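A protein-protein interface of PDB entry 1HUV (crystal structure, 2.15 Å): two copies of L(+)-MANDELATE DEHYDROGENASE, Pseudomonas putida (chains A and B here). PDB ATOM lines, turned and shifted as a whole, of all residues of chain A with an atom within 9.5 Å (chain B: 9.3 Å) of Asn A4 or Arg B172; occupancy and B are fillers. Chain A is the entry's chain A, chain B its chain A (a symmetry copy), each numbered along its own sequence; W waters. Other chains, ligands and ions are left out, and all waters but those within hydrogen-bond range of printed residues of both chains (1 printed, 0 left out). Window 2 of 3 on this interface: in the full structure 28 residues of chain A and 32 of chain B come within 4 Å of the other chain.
The side-chain amide oxygen (OD1) of Asn A4 sits at hydrogen-bond distance from the guanidinium group (NH1) of Arg B172. O of Phe A6 is in hydrogen-bond range of OH of Tyr B164 (2.6 Å). ND2 of Asn A7 is in hydrogen-bond range of OE2 of Glu B166.
The backbone NH (N) of Phe A6 lies within hydrogen-bond range of the side-chain carboxylate (OD2) of Asp A10 (2.8 Å). The side-chain amide oxygen of Asn A7 lies within hydrogen-bond range of the backbone NH of Glu A9. The backbone NH of Asp A10 lies within hydrogen-bond range of the side-chain amide oxygen of Asn A7 (2.8 Å). The guanidinium group of Arg B172 is in hydrogen-bond range of the backbone carbonyl oxygen of Leu B169, at 3.4 Å. O of His B170 lies within hydrogen-bond range of NH1 of Arg B172 (2.9 Å).
His B170 touches Asn A4. O of Leu B169 touches CZ of Phe A6, 3.5 Å away. CD2 of His B170 touches CD2 of Phe A6 (3.3 Å). Asp A10 touches His B170. Tyr B164 touches Leu A328.
Printed residues of chain B within 4 Å of Asn A4: His B170 (3.4 Å) and Arg B172 (2.6 Å). No residue of chain B comes within 4 Å of Leu A5. Glu A9 touches none of the printed residues of chain B. Of the printed residues of chain A, Tyr B164 touches Phe A6 and Leu A328. Of the printed residues of chain A, Glu B166 touches Asn A7. Of the printed residues of chain A, His B170 touches Asn A4 (3.4 Å), Phe A6 (3.3 Å) and Asp A10 (3.9 Å). Arg B172 touches one residue of chain A. The nearest residue of chain B that does not touch Asn A4 is Leu B169 (4.6 Å). The nearest printed residue of chain B that does not touch Leu A328 is Leu B169 (7.5 Å).
Printed residues of chain B that touch a printed residue of chain A: Tyr B164, Glu B166, Leu B169, His B170 and Arg B172. Of the 15 printed residues of chain A, 5 touch a printed residue of chain B. Printed residues of chain A that touch a printed residue of chain B: Asn A4, Phe A6, Asn A7, Asp A10 and Leu A328. Hydrophobic or aromatic side chains of chain A within 4 Å of the printed part of chain B: Phe A6 and Leu A328. Along chain A the printed residues that touch a printed residue of chain B span positions 4 to 328. Among the printed residues, no Asp or Glu carboxylate lies within 4 Å of a Lys or Arg side-chain nitrogen of the other chain.
No position is printed for both chains. Of the 8 pairs that touch across the chains among the printed residues, none has its exchanged pair printed and touching as well.
Water W1 lies within hydrogen-bond range of NE2 of His B170, OD2 of Asp A10 and ND2 of Asn A7.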
ATOM      1  N   ASN A   4     -29.245  -2.155  15.071  1.00  0.00           N
ATOM      2  CA  ASN A   4     -28.121  -1.461  14.376  1.00  0.00           C
ATOM      3  C   ASN A   4     -28.152  -1.708  12.874  1.00  0.00           C
ATOM      4  O   ASN A   4     -27.363  -2.486  12.339  1.00  0.00           O
ATOM      5  CB  ASN A   4     -26.786  -1.929  14.955  1.00  0.00           C
ATOM      6  CG  ASN A   4     -26.560  -1.419  16.362  1.00  0.00           C
ATOM      7  OD1 ASN A   4     -26.370  -0.223  16.575  1.00  0.00           O
ATOM      8  ND2 ASN A   4     -26.591  -2.325  17.333  1.00  0.00           N
ATOM      9  N   LEU A   5     -29.072  -1.036  12.198  1.00  0.00           N
ATOM     10  CA  LEU A   5     -29.217  -1.174  10.761  1.00  0.00           C
ATOM     11  C   LEU A   5     -28.983   0.200  10.137  1.00  0.00           C
ATOM     12  O   LEU A   5     -29.922   0.900   9.766  1.00  0.00           O
ATOM     13  CB  LEU A   5     -30.616  -1.716  10.455  1.00  0.00           C
ATOM     14  CG  LEU A   5     -30.817  -3.109  11.079  1.00  0.00           C
ATOM     15  CD1 LEU A   5     -32.267  -3.546  10.980  1.00  0.00           C
ATOM     16  CD2 LEU A   5     -29.906  -4.104  10.376  1.00  0.00           C
ATOM     17  N   PHE A   6     -27.713   0.573  10.018  1.00  0.00           N
ATOM     18  CA  PHE A   6     -27.356   1.887   9.499  1.00  0.00           C
ATOM     19  C   PHE A   6     -26.738   1.956   8.104  1.00  0.00           C
ATOM     20  O   PHE A   6     -26.528   3.047   7.576  1.00  0.00           O
ATOM     21  CB  PHE A   6     -26.446   2.580  10.516  1.00  0.00           C
ATOM     22  CG  PHE A   6     -27.085   2.745  11.871  1.00  0.00           C
ATOM     23  CD1 PHE A   6     -28.071   3.707  12.080  1.00  0.00           C
ATOM     24  CD2 PHE A   6     -26.734   1.912  12.925  1.00  0.00           C
ATOM     25  CE1 PHE A   6     -28.699   3.836  13.322  1.00  0.00           C
ATOM     26  CE2 PHE A   6     -27.352   2.030  14.173  1.00  0.00           C
ATOM     27  CZ  PHE A   6     -28.336   2.993  14.370  1.00  0.00           C
ATOM     28  N   ASN A   7     -26.444   0.803   7.514  1.00  0.00           N
ATOM     29  CA  ASN A   7     -25.870   0.752   6.175  1.00  0.00           C
ATOM     30  C   ASN A   7     -26.106  -0.639   5.594  1.00  0.00           C
ATOM     31  O   ASN A   7     -26.615  -1.518   6.284  1.00  0.00           O
ATOM     32  CB  ASN A   7     -24.372   1.067   6.212  1.00  0.00           C
ATOM     33  CG  ASN A   7     -23.607   0.132   7.119  1.00  0.00           C
ATOM     34  OD1 ASN A   7     -23.820  -1.080   7.098  1.00  0.00           O
ATOM     35  ND2 ASN A   7     -22.700   0.686   7.916  1.00  0.00           N
ATOM     36  N   VAL A   8     -25.735  -0.835   4.333  1.00  0.00           N
ATOM     37  CA  VAL A   8     -25.938  -2.116   3.657  1.00  0.00           C
ATOM     38  C   VAL A   8     -25.264  -3.295   4.357  1.00  0.00           C
ATOM     39  O   VAL A   8     -25.861  -4.362   4.489  1.00  0.00           O
ATOM     40  CB  VAL A   8     -25.459  -2.043   2.185  1.00  0.00           C
ATOM     41  CG1 VAL A   8     -25.521  -3.425   1.530  1.00  0.00           C
ATOM     42  CG2 VAL A   8     -26.340  -1.064   1.419  1.00  0.00           C
ATOM     43  N   GLU A   9     -24.027  -3.096   4.801  1.00  0.00           N
ATOM     44  CA  GLU A   9     -23.280  -4.140   5.492  1.00  0.00           C
ATOM     45  C   GLU A   9     -24.046  -4.650   6.715  1.00  0.00           C
ATOM     46  O   GLU A   9     -24.010  -5.844   7.014  1.00  0.00           O
ATOM     47  CB  GLU A   9     -21.903  -3.605   5.903  1.00  0.00           C
ATOM     48  CG  GLU A   9     -21.090  -4.519   6.816  1.00  0.00           C
ATOM     49  CD  GLU A   9     -20.696  -5.847   6.183  1.00  0.00           C
ATOM     50  OE1 GLU A   9     -20.965  -6.069   4.981  1.00  0.00           O
ATOM     51  OE2 GLU A   9     -20.101  -6.676   6.900  1.00  0.00           O
ATOM     52  N   ASP A  10     -24.739  -3.750   7.414  1.00  0.00           N
ATOM     53  CA  ASP A  10     -25.528  -4.138   8.584  1.00  0.00           C
ATOM     54  C   ASP A  10     -26.649  -5.079   8.151  1.00  0.00           C
ATOM     55  O   ASP A  10     -27.012  -6.007   8.879  1.00  0.00           O
ATOM     56  CB  ASP A  10     -26.150  -2.916   9.281  1.00  0.00           C
ATOM     57  CG  ASP A  10     -25.139  -2.107  10.083  1.00  0.00           C
ATOM     58  OD1 ASP A  10     -24.052  -2.637  10.382  1.00  0.00           O
ATOM     59  OD2 ASP A  10     -25.442  -0.944  10.429  1.00  0.00           O
ATOM     60  N   TYR A  11     -27.210  -4.832   6.970  1.00  0.00           N
ATOM     61  CA  TYR A  11     -28.276  -5.687   6.479  1.00  0.00           C
ATOM     62  C   TYR A  11     -27.713  -7.032   6.036  1.00  0.00           C
ATOM     63  O   TYR A  11     -28.370  -8.058   6.194  1.00  0.00           O
ATOM     64  CB  TYR A  11     -29.063  -4.997   5.351  1.00  0.00           C
ATOM     65  CG  TYR A  11     -30.100  -4.034   5.895  1.00  0.00           C
ATOM     66  CD1 TYR A  11     -29.759  -2.726   6.238  1.00  0.00           C
ATOM     67  CD2 TYR A  11     -31.398  -4.468   6.175  1.00  0.00           C
ATOM     68  CE1 TYR A  11     -30.680  -1.876   6.855  1.00  0.00           C
ATOM     69  CE2 TYR A  11     -32.327  -3.627   6.792  1.00  0.00           C
ATOM     70  CZ  TYR A  11     -31.959  -2.336   7.132  1.00  0.00           C
ATOM     71  OH  TYR A  11     -32.859  -1.511   7.766  1.00  0.00           O
ATOM     72  N   ARG A  12     -26.493  -7.036   5.505  1.00  0.00           N
ATOM     73  CA  ARG A  12     -25.877  -8.296   5.098  1.00  0.00           C
ATOM     74  C   ARG A  12     -25.731  -9.164   6.350  1.00  0.00           C
ATOM     75  O   ARG A  12     -26.094 -10.341   6.347  1.00  0.00           O
ATOM     76  CB  ARG A  12     -24.485  -8.078   4.482  1.00  0.00           C
ATOM     77  CG  ARG A  12     -23.831  -9.389   4.035  1.00  0.00           C
ATOM     78  CD  ARG A  12     -22.331  -9.266   3.778  1.00  0.00           C
ATOM     79  NE  ARG A  12     -21.579  -8.968   4.996  1.00  0.00           N
ATOM     80  CZ  ARG A  12     -21.432  -9.804   6.021  1.00  0.00           C
ATOM     81  NH1 ARG A  12     -21.980 -11.016   5.995  1.00  0.00           N
ATOM     82  NH2 ARG A  12     -20.742  -9.423   7.085  1.00  0.00           N
ATOM     83  N   LYS A  13     -25.202  -8.569   7.419  1.00  0.00           N
ATOM     84  CA  LYS A  13     -25.001  -9.276   8.686  1.00  0.00           C
ATOM     85  C   LYS A  13     -26.286  -9.896   9.220  1.00  0.00           C
ATOM     86  O   LYS A  13     -26.293 -11.044   9.662  1.00  0.00           O
ATOM     87  CB  LYS A  13     -24.425  -8.327   9.736  1.00  0.00           C
ATOM     88  CG  LYS A  13     -23.000  -7.890   9.453  1.00  0.00           C
ATOM     89  CD  LYS A  13     -22.521  -6.869  10.470  1.00  0.00           C
ATOM     90  CE  LYS A  13     -21.094  -6.436  10.173  1.00  0.00           C
ATOM     91  NZ  LYS A  13     -20.630  -5.383  11.119  1.00  0.00           N
ATOM     92  N   LEU A  14     -27.369  -9.127   9.192  1.00  0.00           N
ATOM     93  CA  LEU A  14     -28.650  -9.619   9.671  1.00  0.00           C
ATOM     94  C   LEU A  14     -29.176 -10.704   8.729  1.00  0.00           C
ATOM     95  O   LEU A  14     -29.790 -11.675   9.168  1.00  0.00           O
ATOM     96  CB  LEU A  14     -29.653  -8.464   9.774  1.00  0.00           C
ATOM     97  CG  LEU A  14     -31.049  -8.821  10.294  1.00  0.00           C
ATOM     98  CD1 LEU A  14     -30.926  -9.659  11.564  1.00  0.00           C
ATOM     99  CD2 LEU A  14     -31.844  -7.543  10.552  1.00  0.00           C
ATOM    100  N   LYS A  17     -27.649 -14.008   9.396  1.00  0.00           N
ATOM    101  CA  LYS A  17     -28.213 -14.615  10.597  1.00  0.00           C
ATOM    102  C   LYS A  17     -29.542 -15.312  10.339  1.00  0.00           C
ATOM    103  O   LYS A  17     -29.837 -16.328  10.956  1.00  0.00           O
ATOM    104  CB  LYS A  17     -28.447 -13.561  11.676  1.00  0.00           C
ATOM    105  CG  LYS A  17     -27.213 -13.099  12.417  1.00  0.00           C
ATOM    106  CD  LYS A  17     -27.599 -12.016  13.402  1.00  0.00           C
ATOM    107  CE  LYS A  17     -26.385 -11.350  14.012  1.00  0.00           C
ATOM    108  NZ  LYS A  17     -26.804 -10.142  14.773  1.00  0.00           N
ATOM    109  N   ARG A 317     -35.408  -8.527   6.235  1.00  0.00           N
ATOM    110  CA  ARG A 317     -36.707  -8.044   6.697  1.00  0.00           C
ATOM    111  C   ARG A 317     -37.779  -7.886   5.625  1.00  0.00           C
ATOM    112  O   ARG A 317     -38.648  -7.018   5.744  1.00  0.00           O
ATOM    113  CB  ARG A 317     -36.542  -6.699   7.414  1.00  0.00           C
ATOM    114  CG  ARG A 317     -35.485  -6.660   8.513  1.00  0.00           C
ATOM    115  CD  ARG A 317     -35.640  -5.391   9.354  1.00  0.00           C
ATOM    116  NE  ARG A 317     -36.614  -5.597  10.423  1.00  0.00           N
ATOM    117  CZ  ARG A 317     -37.573  -4.740  10.757  1.00  0.00           C
ATOM    118  NH1 ARG A 317     -37.710  -3.590  10.108  1.00  0.00           N
ATOM    119  NH2 ARG A 317     -38.408  -5.044  11.742  1.00  0.00           N
ATOM    120  N   GLU A 324     -36.131  -0.036   3.578  1.00  0.00           N
ATOM    121  CA  GLU A 324     -35.105   0.490   4.463  1.00  0.00           C
ATOM    122  C   GLU A 324     -33.760   0.650   3.771  1.00  0.00           C
ATOM    123  O   GLU A 324     -33.111   1.689   3.909  1.00  0.00           O
ATOM    124  CB  GLU A 324     -34.986  -0.398   5.709  1.00  0.00           C
ATOM    125  CG  GLU A 324     -36.240  -0.328   6.594  1.00  0.00           C
ATOM    126  CD  GLU A 324     -36.219  -1.306   7.758  1.00  0.00           C
ATOM    127  OE1 GLU A 324     -35.337  -2.188   7.784  1.00  0.00           O
ATOM    128  OE2 GLU A 324     -37.093  -1.197   8.641  1.00  0.00           O
ATOM    129  N   LEU A 328     -31.858   4.362   3.128  1.00  0.00           N
ATOM    130  CA  LEU A 328     -30.506   4.636   3.615  1.00  0.00           C
ATOM    131  C   LEU A 328     -29.634   5.016   2.427  1.00  0.00           C
ATOM    132  O   LEU A 328     -28.896   6.000   2.479  1.00  0.00           O
ATOM    133  CB  LEU A 328     -29.896   3.409   4.310  1.00  0.00           C
ATOM    134  CG  LEU A 328     -30.448   3.052   5.692  1.00  0.00           C
ATOM    135  CD1 LEU A 328     -29.839   1.741   6.181  1.00  0.00           C
ATOM    136  CD2 LEU A 328     -30.143   4.183   6.660  1.00  0.00           C
ATOM    137  N   MET B  22     -18.102   5.447  24.843  1.00  0.00           N
ATOM    138  CA  MET B  22     -18.941   6.295  24.000  1.00  0.00           C
ATOM    139  C   MET B  22     -18.297   7.640  23.673  1.00  0.00           C
ATOM    140  O   MET B  22     -18.477   8.180  22.574  1.00  0.00           O
ATOM    141  CB  MET B  22     -20.269   6.514  24.711  1.00  0.00           C
ATOM    142  CG  MET B  22     -21.256   7.415  24.016  1.00  0.00           C
ATOM    143  SD  MET B  22     -22.776   7.526  25.026  1.00  0.00           S
ATOM    144  CE  MET B  22     -23.056   5.737  25.348  1.00  0.00           C
ATOM    145  N   ASP B  25     -15.183   6.810  21.433  1.00  0.00           N
ATOM    146  CA  ASP B  25     -15.603   6.533  20.056  1.00  0.00           C
ATOM    147  C   ASP B  25     -15.977   7.827  19.337  1.00  0.00           C
ATOM    148  O   ASP B  25     -15.673   8.011  18.158  1.00  0.00           O
ATOM    149  CB  ASP B  25     -16.796   5.567  20.028  1.00  0.00           C
ATOM    150  CG  ASP B  25     -16.377   4.110  20.157  1.00  0.00           C
ATOM    151  OD1 ASP B  25     -15.181   3.808  19.951  1.00  0.00           O
ATOM    152  OD2 ASP B  25     -17.248   3.261  20.448  1.00  0.00           O
ATOM    153  N   TYR B  26     -16.643   8.722  20.056  1.00  0.00           N
ATOM    154  CA  TYR B  26     -17.037  10.002  19.495  1.00  0.00           C
ATOM    155  C   TYR B  26     -15.803  10.824  19.086  1.00  0.00           C
ATOM    156  O   TYR B  26     -15.855  11.592  18.131  1.00  0.00           O
ATOM    157  CB  TYR B  26     -17.866  10.773  20.523  1.00  0.00           C
ATOM    158  CG  TYR B  26     -17.640  12.259  20.476  1.00  0.00           C
ATOM    159  CD1 TYR B  26     -18.265  13.051  19.517  1.00  0.00           C
ATOM    160  CD2 TYR B  26     -16.749  12.867  21.360  1.00  0.00           C
ATOM    161  CE1 TYR B  26     -18.008  14.414  19.436  1.00  0.00           C
ATOM    162  CE2 TYR B  26     -16.484  14.228  21.287  1.00  0.00           C
ATOM    163  CZ  TYR B  26     -17.115  14.995  20.322  1.00  0.00           C
ATOM    164  OH  TYR B  26     -16.850  16.341  20.237  1.00  0.00           O
ATOM    165  N   TYR B 164     -21.694  11.136   8.490  1.00  0.00           N
ATOM    166  CA  TYR B 164     -22.331   9.893   8.908  1.00  0.00           C
ATOM    167  C   TYR B 164     -21.328   9.040   9.685  1.00  0.00           C
ATOM    168  O   TYR B 164     -20.671   8.171   9.116  1.00  0.00           O
ATOM    169  CB  TYR B 164     -22.838   9.129   7.680  1.00  0.00           C
ATOM    170  CG  TYR B 164     -23.945   8.134   7.965  1.00  0.00           C
ATOM    171  CD1 TYR B 164     -25.226   8.566   8.298  1.00  0.00           C
ATOM    172  CD2 TYR B 164     -23.720   6.763   7.873  1.00  0.00           C
ATOM    173  CE1 TYR B 164     -26.259   7.661   8.525  1.00  0.00           C
ATOM    174  CE2 TYR B 164     -24.749   5.845   8.101  1.00  0.00           C
ATOM    175  CZ  TYR B 164     -26.018   6.301   8.425  1.00  0.00           C
ATOM    176  OH  TYR B 164     -27.045   5.405   8.642  1.00  0.00           O
ATOM    177  N   ARG B 165     -21.216   9.301  10.986  1.00  0.00           N
ATOM    178  CA  ARG B 165     -20.297   8.562  11.845  1.00  0.00           C
ATOM    179  C   ARG B 165     -21.053   7.450  12.539  1.00  0.00           C
ATOM    180  O   ARG B 165     -21.807   7.674  13.487  1.00  0.00           O
ATOM    181  CB  ARG B 165     -19.649   9.507  12.854  1.00  0.00           C
ATOM    182  CG  ARG B 165     -18.718  10.511  12.189  1.00  0.00           C
ATOM    183  CD  ARG B 165     -18.249  11.570  13.160  1.00  0.00           C
ATOM    184  NE  ARG B 165     -18.306  12.873  12.529  1.00  0.00           N
ATOM    185  CZ  ARG B 165     -18.556  14.001  13.175  1.00  0.00           C
ATOM    186  NH1 ARG B 165     -18.769  13.984  14.485  1.00  0.00           N
ATOM    187  NH2 ARG B 165     -18.616  15.137  12.494  1.00  0.00           N
ATOM    188  N   GLU B 166     -20.822   6.239  12.054  1.00  0.00           N
ATOM    189  CA  GLU B 166     -21.512   5.070  12.552  1.00  0.00           C
ATOM    190  C   GLU B 166     -21.187   4.620  13.976  1.00  0.00           C
ATOM    191  O   GLU B 166     -22.002   3.937  14.597  1.00  0.00           O
ATOM    192  CB  GLU B 166     -21.348   3.945  11.521  1.00  0.00           C
ATOM    193  CG  GLU B 166     -21.785   4.457  10.136  1.00  0.00           C
ATOM    194  CD  GLU B 166     -21.575   3.494   8.999  1.00  0.00           C
ATOM    195  OE1 GLU B 166     -20.539   2.800   8.968  1.00  0.00           O
ATOM    196  OE2 GLU B 166     -22.442   3.439   8.098  1.00  0.00           O
ATOM    197  N   ARG B 167     -20.039   5.011  14.521  1.00  0.00           N
ATOM    198  CA  ARG B 167     -19.759   4.618  15.894  1.00  0.00           C
ATOM    199  C   ARG B 167     -20.780   5.306  16.793  1.00  0.00           C
ATOM    200  O   ARG B 167     -21.306   4.691  17.720  1.00  0.00           O
ATOM    201  CB  ARG B 167     -18.356   5.028  16.332  1.00  0.00           C
ATOM    202  CG  ARG B 167     -17.233   4.280  15.659  1.00  0.00           C
ATOM    203  CD  ARG B 167     -15.949   4.435  16.461  1.00  0.00           C
ATOM    204  NE  ARG B 167     -14.776   4.089  15.675  1.00  0.00           N
ATOM    205  CZ  ARG B 167     -13.572   3.864  16.191  1.00  0.00           C
ATOM    206  NH1 ARG B 167     -13.379   3.941  17.506  1.00  0.00           N
ATOM    207  NH2 ARG B 167     -12.559   3.573  15.382  1.00  0.00           N
ATOM    208  N   ASP B 168     -21.048   6.581  16.511  1.00  0.00           N
ATOM    209  CA  ASP B 168     -22.002   7.374  17.286  1.00  0.00           C
ATOM    210  C   ASP B 168     -23.416   6.821  17.128  1.00  0.00           C
ATOM    211  O   ASP B 168     -24.194   6.807  18.082  1.00  0.00           O
ATOM    212  CB  ASP B 168     -22.008   8.844  16.831  1.00  0.00           C
ATOM    213  CG  ASP B 168     -20.724   9.575  17.153  1.00  0.00           C
ATOM    214  OD1 ASP B 168     -19.949   9.120  18.023  1.00  0.00           O
ATOM    215  OD2 ASP B 168     -20.487  10.638  16.537  1.00  0.00           O
ATOM    216  N   LEU B 169     -23.751   6.393  15.915  1.00  0.00           N
ATOM    217  CA  LEU B 169     -25.073   5.845  15.642  1.00  0.00           C
ATOM    218  C   LEU B 169     -25.286   4.549  16.418  1.00  0.00           C
ATOM    219  O   LEU B 169     -26.367   4.327  16.962  1.00  0.00           O
ATOM    220  CB  LEU B 169     -25.253   5.620  14.136  1.00  0.00           C
ATOM    221  CG  LEU B 169     -25.343   6.894  13.300  1.00  0.00           C
ATOM    222  CD1 LEU B 169     -25.305   6.557  11.820  1.00  0.00           C
ATOM    223  CD2 LEU B 169     -26.616   7.641  13.661  1.00  0.00           C
ATOM    224  N   HIS B 170     -24.256   3.708  16.481  1.00  0.00           N
ATOM    225  CA  HIS B 170     -24.352   2.450  17.218  1.00  0.00           C
ATOM    226  C   HIS B 170     -24.404   2.683  18.722  1.00  0.00           C
ATOM    227  O   HIS B 170     -25.009   1.894  19.448  1.00  0.00           O
ATOM    228  CB  HIS B 170     -23.164   1.534  16.913  1.00  0.00           C
ATOM    229  CG  HIS B 170     -23.132   1.024  15.505  1.00  0.00           C
ATOM    230  ND1 HIS B 170     -22.298   0.002  15.108  1.00  0.00           N
ATOM    231  CD2 HIS B 170     -23.817   1.401  14.400  1.00  0.00           C
ATOM    232  CE1 HIS B 170     -22.471  -0.230  13.817  1.00  0.00           C
ATOM    233  NE2 HIS B 170     -23.388   0.606  13.364  1.00  0.00           N
ATOM    234  N   ASN B 171     -23.757   3.748  19.191  1.00  0.00           N
ATOM    235  CA  ASN B 171     -23.744   4.062  20.616  1.00  0.00           C
ATOM    236  C   ASN B 171     -24.861   5.037  20.984  1.00  0.00           C
ATOM    237  O   ASN B 171     -24.960   5.446  22.136  1.00  0.00           O
ATOM    238  CB  ASN B 171     -22.412   4.705  21.042  1.00  0.00           C
ATOM    239  CG  ASN B 171     -21.206   3.809  20.806  1.00  0.00           C
ATOM    240  OD1 ASN B 171     -21.289   2.582  20.907  1.00  0.00           O
ATOM    241  ND2 ASN B 171     -20.066   4.431  20.514  1.00  0.00           N
ATOM    242  N   ARG B 172     -25.697   5.410  20.019  1.00  0.00           N
ATOM    243  CA  ARG B 172     -26.770   6.363  20.291  1.00  0.00           C
ATOM    244  C   ARG B 172     -26.177   7.564  21.024  1.00  0.00           C
ATOM    245  O   ARG B 172     -26.814   8.141  21.905  1.00  0.00           O
ATOM    246  CB  ARG B 172     -27.855   5.719  21.166  1.00  0.00           C
ATOM    247  CG  ARG B 172     -28.866   4.858  20.411  1.00  0.00           C
ATOM    248  CD  ARG B 172     -28.218   3.653  19.748  1.00  0.00           C
ATOM    249  NE  ARG B 172     -29.186   2.857  19.006  1.00  0.00           N
ATOM    250  CZ  ARG B 172     -28.870   1.798  18.266  1.00  0.00           C
ATOM    251  NH1 ARG B 172     -27.604   1.412  18.171  1.00  0.00           N
ATOM    252  NH2 ARG B 172     -29.821   1.130  17.622  1.00  0.00           N
ATOM    253  N   PHE B 173     -24.957   7.939  20.644  1.00  0.00           N
ATOM    254  CA  PHE B 173     -24.264   9.052  21.282  1.00  0.00           C
ATOM    255  C   PHE B 173     -25.127  10.278  21.492  1.00  0.00           C
ATOM    256  O   PHE B 173     -25.584  10.909  20.540  1.00  0.00           O
ATOM    257  CB  PHE B 173     -23.024   9.473  20.487  1.00  0.00           C
ATOM    258  CG  PHE B 173     -22.199  10.529  21.179  1.00  0.00           C
ATOM    259  CD1 PHE B 173     -21.497  10.227  22.341  1.00  0.00           C
ATOM    260  CD2 PHE B 173     -22.146  11.831  20.689  1.00  0.00           C
ATOM    261  CE1 PHE B 173     -20.753  11.200  23.004  1.00  0.00           C
ATOM    262  CE2 PHE B 173     -21.402  12.816  21.348  1.00  0.00           C
ATOM    263  CZ  PHE B 173     -20.705  12.498  22.508  1.00  0.00           C
ATOM    264  N   LYS B 174     -25.326  10.606  22.762  1.00  0.00           N
ATOM    265  CA  LYS B 174     -26.101  11.763  23.171  1.00  0.00           C
ATOM    266  C   LYS B 174     -25.116  12.718  23.846  1.00  0.00           C
ATOM    267  O   LYS B 174     -24.494  12.358  24.849  1.00  0.00           O
ATOM    268  CB  LYS B 174     -27.193  11.340  24.163  1.00  0.00           C
ATOM    269  N   ILE B 175     -24.957  13.914  23.278  1.00  0.00           N
ATOM    270  CA  ILE B 175     -24.048  14.913  23.823  1.00  0.00           C
ATOM    271  C   ILE B 175     -24.216  14.968  25.337  1.00  0.00           C
ATOM    272  O   ILE B 175     -25.268  15.366  25.842  1.00  0.00           O
ATOM    273  N   PRO B 176     -23.175  14.545  26.091  1.00  0.00           N
ATOM    274  CA  PRO B 176     -23.234  14.548  27.567  1.00  0.00           C
ATOM    275  C   PRO B 176     -24.054  15.716  28.170  1.00  0.00           C
ATOM    276  O   PRO B 176     -24.037  16.851  27.670  1.00  0.00           O
ATOM    277  CB  PRO B 176     -21.780  14.583  27.995  1.00  0.00           C
ATOM    278  CG  PRO B 176     -21.006  14.031  26.836  1.00  0.00           C
ATOM    279  CD  PRO B 176     -21.814  14.287  25.582  1.00  0.00           C
HETATM  280  O   HOH W   1     -22.923   0.311  11.024  1.00  0.00           O
